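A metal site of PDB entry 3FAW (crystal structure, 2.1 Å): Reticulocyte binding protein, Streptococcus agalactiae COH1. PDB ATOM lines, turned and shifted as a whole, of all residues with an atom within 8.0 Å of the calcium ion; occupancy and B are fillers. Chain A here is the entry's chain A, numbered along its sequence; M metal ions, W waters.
The backbone NH (N) of Asp 339 lies within hydrogen-bond range of the side-chain carboxylate (OD2) of Asp 665, at 2.8 Å.
O of Asp 665 sits at hydrogen-bond distance from N of Ser 338, at 3.2 Å.
O of Ser 338 is in hydrogen-bond range of ND2 of Asn 340.
Within 4 Å of the calcium ion: Asn 340, Tyr 342 and Asp 665.
The calcium ion is bound by the backbone carbonyl oxygen of Tyr 342 (2.3 Å), the side-chain carboxylate of Asp 665 (2.4 Å), water W1 (2.4 Å), the backbone carbonyl oxygen of Asn 340 (2.4 Å), water W2 (2.5 Å), water W3 (2.6 Å) and water W4 (2.7 Å).
Water W2 lies within hydrogen-bond range of the backbone carbonyl oxygen of Tyr 323 (2.7 Å) and the backbone carbonyl oxygen of Asn 341 (2.7 Å).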
ATOM      1  N   TYR A 321      21.738  27.636   0.943  1.00  0.00           N
ATOM      2  CA  TYR A 321      22.365  27.888   2.245  1.00  0.00           C
ATOM      3  C   TYR A 321      22.749  26.581   2.916  1.00  0.00           C
ATOM      4  O   TYR A 321      22.186  25.529   2.608  1.00  0.00           O
ATOM      5  CB  TYR A 321      21.466  28.750   3.150  1.00  0.00           C
ATOM      6  CG  TYR A 321      20.030  28.288   3.306  1.00  0.00           C
ATOM      7  CD1 TYR A 321      19.671  27.398   4.312  1.00  0.00           C
ATOM      8  CD2 TYR A 321      19.031  28.794   2.483  1.00  0.00           C
ATOM      9  CE1 TYR A 321      18.349  26.990   4.485  1.00  0.00           C
ATOM     10  CE2 TYR A 321      17.695  28.387   2.642  1.00  0.00           C
ATOM     11  CZ  TYR A 321      17.364  27.488   3.647  1.00  0.00           C
ATOM     12  OH  TYR A 321      16.060  27.092   3.816  1.00  0.00           O
ATOM     13  N   TYR A 323      23.428  25.348   6.495  1.00  0.00           N
ATOM     14  CA  TYR A 323      22.891  24.650   7.662  1.00  0.00           C
ATOM     15  C   TYR A 323      21.425  24.273   7.470  1.00  0.00           C
ATOM     16  O   TYR A 323      20.518  25.033   7.822  1.00  0.00           O
ATOM     17  CB  TYR A 323      23.073  25.488   8.925  1.00  0.00           C
ATOM     18  CG  TYR A 323      24.516  25.773   9.263  1.00  0.00           C
ATOM     19  CD1 TYR A 323      25.036  27.058   9.144  1.00  0.00           C
ATOM     20  CD2 TYR A 323      25.362  24.757   9.698  1.00  0.00           C
ATOM     21  CE1 TYR A 323      26.361  27.331   9.458  1.00  0.00           C
ATOM     22  CE2 TYR A 323      26.698  25.022  10.014  1.00  0.00           C
ATOM     23  CZ  TYR A 323      27.187  26.310   9.884  1.00  0.00           C
ATOM     24  OH  TYR A 323      28.501  26.591  10.196  1.00  0.00           O
ATOM     25  N   VAL A 324      21.204  23.096   6.896  1.00  0.00           N
ATOM     26  CA  VAL A 324      19.855  22.633   6.551  1.00  0.00           C
ATOM     27  C   VAL A 324      19.856  21.151   6.160  1.00  0.00           C
ATOM     28  O   VAL A 324      20.870  20.612   5.699  1.00  0.00           O
ATOM     29  CB  VAL A 324      19.270  23.453   5.371  1.00  0.00           C
ATOM     30  CG1 VAL A 324      19.974  23.088   4.068  1.00  0.00           C
ATOM     31  CG2 VAL A 324      17.760  23.231   5.247  1.00  0.00           C
ATOM     32  N   ASN A 325      18.712  20.507   6.366  1.00  0.00           N
ATOM     33  CA  ASN A 325      18.424  19.175   5.835  1.00  0.00           C
ATOM     34  C   ASN A 325      17.215  19.300   4.930  1.00  0.00           C
ATOM     35  O   ASN A 325      16.083  19.402   5.398  1.00  0.00           O
ATOM     36  CB  ASN A 325      18.149  18.161   6.948  1.00  0.00           C
ATOM     37  CG  ASN A 325      17.831  16.760   6.414  1.00  0.00           C
ATOM     38  OD1 ASN A 325      17.921  16.496   5.211  1.00  0.00           O
ATOM     39  ND2 ASN A 325      17.480  15.853   7.311  1.00  0.00           N
ATOM     40  N   SER A 338      15.664  27.860  19.022  1.00  0.00           N
ATOM     41  CA  SER A 338      16.951  27.285  18.653  1.00  0.00           C
ATOM     42  C   SER A 338      16.785  25.837  18.205  1.00  0.00           C
ATOM     43  O   SER A 338      15.809  25.176  18.568  1.00  0.00           O
ATOM     44  CB  SER A 338      17.926  27.338  19.834  1.00  0.00           C
ATOM     45  OG  SER A 338      18.378  28.661  20.070  1.00  0.00           O
ATOM     46  N   ASP A 339      17.762  25.356  17.430  1.00  0.00           N
ATOM     47  CA  ASP A 339      17.866  23.951  17.053  1.00  0.00           C
ATOM     48  C   ASP A 339      16.661  23.474  16.235  1.00  0.00           C
ATOM     49  O   ASP A 339      16.047  22.466  16.537  1.00  0.00           O
ATOM     50  CB  ASP A 339      18.082  23.074  18.304  1.00  0.00           C
ATOM     51  CG  ASP A 339      18.598  21.682  17.982  1.00  0.00           C
ATOM     52  OD1 ASP A 339      19.119  21.445  16.871  1.00  0.00           O
ATOM     53  OD2 ASP A 339      18.481  20.802  18.857  1.00  0.00           O
ATOM     54  N   ASN A 340      16.343  24.239  15.195  1.00  0.00           N
ATOM     55  CA  ASN A 340      15.311  23.856  14.237  1.00  0.00           C
ATOM     56  C   ASN A 340      15.893  23.761  12.831  1.00  0.00           C
ATOM     57  O   ASN A 340      16.822  24.498  12.492  1.00  0.00           O
ATOM     58  CB  ASN A 340      14.171  24.869  14.270  1.00  0.00           C
ATOM     59  CG  ASN A 340      13.387  24.808  15.556  1.00  0.00           C
ATOM     60  OD1 ASN A 340      12.486  23.985  15.704  1.00  0.00           O
ATOM     61  ND2 ASN A 340      13.723  25.680  16.509  1.00  0.00           N
ATOM     62  N   ASN A 341      15.335  22.865  12.031  1.00  0.00           N
ATOM     63  CA  ASN A 341      15.737  22.736  10.620  1.00  0.00           C
ATOM     64  C   ASN A 341      15.476  24.030   9.853  1.00  0.00           C
ATOM     65  O   ASN A 341      16.089  24.291   8.823  1.00  0.00           O
ATOM     66  CB  ASN A 341      14.995  21.569   9.961  1.00  0.00           C
ATOM     67  CG  ASN A 341      15.582  21.184   8.603  1.00  0.00           C
ATOM     68  OD1 ASN A 341      16.891  21.177   8.518  1.00  0.00           O
ATOM     69  ND2 ASN A 341      14.850  20.895   7.660  1.00  0.00           N
ATOM     70  N   TYR A 342      14.532  24.820  10.373  1.00  0.00           N
ATOM     71  CA  TYR A 342      14.277  26.170   9.873  1.00  0.00           C
ATOM     72  C   TYR A 342      15.551  27.003   9.733  1.00  0.00           C
ATOM     73  O   TYR A 342      16.445  26.918  10.560  1.00  0.00           O
ATOM     74  CB  TYR A 342      13.321  26.889  10.827  1.00  0.00           C
ATOM     75  CG  TYR A 342      12.899  28.247  10.312  1.00  0.00           C
ATOM     76  CD1 TYR A 342      11.812  28.363   9.469  1.00  0.00           C
ATOM     77  CD2 TYR A 342      13.611  29.393  10.646  1.00  0.00           C
ATOM     78  CE1 TYR A 342      11.424  29.591   8.982  1.00  0.00           C
ATOM     79  CE2 TYR A 342      13.224  30.635  10.159  1.00  0.00           C
ATOM     80  CZ  TYR A 342      12.131  30.724   9.334  1.00  0.00           C
ATOM     81  OH  TYR A 342      11.741  31.945   8.835  1.00  0.00           O
ATOM     82  N   ASN A 343      15.592  27.827   8.689  1.00  0.00           N
ATOM     83  CA  ASN A 343      16.720  28.727   8.458  1.00  0.00           C
ATOM     84  C   ASN A 343      16.267  29.878   7.578  1.00  0.00           C
ATOM     85  O   ASN A 343      15.642  29.641   6.544  1.00  0.00           O
ATOM     86  CB  ASN A 343      17.868  27.956   7.777  1.00  0.00           C
ATOM     87  CG  ASN A 343      19.210  28.682   7.845  1.00  0.00           C
ATOM     88  OD1 ASN A 343      19.285  29.901   7.973  1.00  0.00           O
ATOM     89  ND2 ASN A 343      20.284  27.914   7.738  1.00  0.00           N
ATOM     90  N   TRP A 344      16.559  31.121   7.985  1.00  0.00           N
ATOM     91  CA  TRP A 344      16.273  32.294   7.137  1.00  0.00           C
ATOM     92  C   TRP A 344      17.016  32.187   5.811  1.00  0.00           C
ATOM     93  O   TRP A 344      16.467  32.525   4.764  1.00  0.00           O
ATOM     94  CB  TRP A 344      16.663  33.614   7.821  1.00  0.00           C
ATOM     95  CG  TRP A 344      15.684  34.152   8.815  1.00  0.00           C
ATOM     96  CD1 TRP A 344      14.348  33.863   8.909  1.00  0.00           C
ATOM     97  CD2 TRP A 344      15.947  35.124   9.833  1.00  0.00           C
ATOM     98  NE1 TRP A 344      13.780  34.570   9.939  1.00  0.00           N
ATOM     99  CE2 TRP A 344      14.742  35.346  10.523  1.00  0.00           C
ATOM    100  CE3 TRP A 344      17.110  35.812  10.237  1.00  0.00           C
ATOM    101  CZ2 TRP A 344      14.648  36.239  11.598  1.00  0.00           C
ATOM    102  CZ3 TRP A 344      17.003  36.699  11.310  1.00  0.00           C
ATOM    103  CH2 TRP A 344      15.787  36.901  11.982  1.00  0.00           C
ATOM    104  N   ASP A 347      23.336  31.826   5.506  1.00  0.00           N
ATOM    105  CA  ASP A 347      24.530  30.982   5.585  1.00  0.00           C
ATOM    106  C   ASP A 347      24.873  30.496   4.169  1.00  0.00           C
ATOM    107  O   ASP A 347      24.715  29.308   3.857  1.00  0.00           O
ATOM    108  CB  ASP A 347      24.272  29.789   6.498  1.00  0.00           C
ATOM    109  CG  ASP A 347      23.755  30.204   7.871  1.00  0.00           C
ATOM    110  OD1 ASP A 347      24.406  31.052   8.518  1.00  0.00           O
ATOM    111  OD2 ASP A 347      22.704  29.680   8.303  1.00  0.00           O
ATOM    112  N   SER A 663      14.531  35.353  15.120  1.00  0.00           N
ATOM    113  CA  SER A 663      13.916  34.045  14.879  1.00  0.00           C
ATOM    114  C   SER A 663      14.560  33.243  13.737  1.00  0.00           C
ATOM    115  O   SER A 663      13.910  32.402  13.119  1.00  0.00           O
ATOM    116  CB  SER A 663      12.405  34.224  14.638  1.00  0.00           C
ATOM    117  OG  SER A 663      12.149  34.965  13.462  1.00  0.00           O
ATOM    118  N   TYR A 664      15.846  33.481  13.490  1.00  0.00           N
ATOM    119  CA  TYR A 664      16.575  32.794  12.427  1.00  0.00           C
ATOM    120  C   TYR A 664      16.622  31.267  12.585  1.00  0.00           C
ATOM    121  O   TYR A 664      16.690  30.550  11.603  1.00  0.00           O
ATOM    122  CB  TYR A 664      17.997  33.358  12.305  1.00  0.00           C
ATOM    123  CG  TYR A 664      19.022  32.732  13.237  1.00  0.00           C
ATOM    124  CD1 TYR A 664      20.048  31.928  12.749  1.00  0.00           C
ATOM    125  CD2 TYR A 664      18.965  32.941  14.618  1.00  0.00           C
ATOM    126  CE1 TYR A 664      20.980  31.358  13.593  1.00  0.00           C
ATOM    127  CE2 TYR A 664      19.894  32.372  15.479  1.00  0.00           C
ATOM    128  CZ  TYR A 664      20.897  31.576  14.957  1.00  0.00           C
ATOM    129  OH  TYR A 664      21.835  31.012  15.796  1.00  0.00           O
ATOM    130  N   ASP A 665      16.588  30.796  13.842  1.00  0.00           N
ATOM    131  CA  ASP A 665      16.682  29.370  14.172  1.00  0.00           C
ATOM    132  C   ASP A 665      15.472  28.923  15.026  1.00  0.00           C
ATOM    133  O   ASP A 665      15.567  28.008  15.855  1.00  0.00           O
ATOM    134  CB  ASP A 665      18.007  29.102  14.909  1.00  0.00           C
ATOM    135  CG  ASP A 665      18.414  27.623  14.918  1.00  0.00           C
ATOM    136  OD1 ASP A 665      18.042  26.869  13.995  1.00  0.00           O
ATOM    137  OD2 ASP A 665      19.133  27.224  15.860  1.00  0.00           O
ATOM    138  N   SER A 666      14.330  29.581  14.812  1.00  0.00           N
ATOM    139  CA  SER A 666      13.114  29.308  15.569  1.00  0.00           C
ATOM    140  C   SER A 666      12.189  28.381  14.781  1.00  0.00           C
ATOM    141  O   SER A 666      12.334  28.239  13.558  1.00  0.00           O
ATOM    142  CB  SER A 666      12.358  30.608  15.886  1.00  0.00           C
ATOM    143  OG  SER A 666      13.057  31.397  16.837  1.00  0.00           O
HETATM  144 CA    CA M   1      18.331  26.235  11.728  1.00  0.00          CA
HETATM  145  O   HOH W   1      18.540  28.631  11.480  1.00  0.00           O
HETATM  146  O   HOH W   2      18.578  24.915   9.661  1.00  0.00           O
HETATM  147  O   HOH W   3      20.823  26.448  11.187  1.00  0.00           O
HETATM  148  O   HOH W   4      19.509  24.134  12.956  1.00  0.00           O
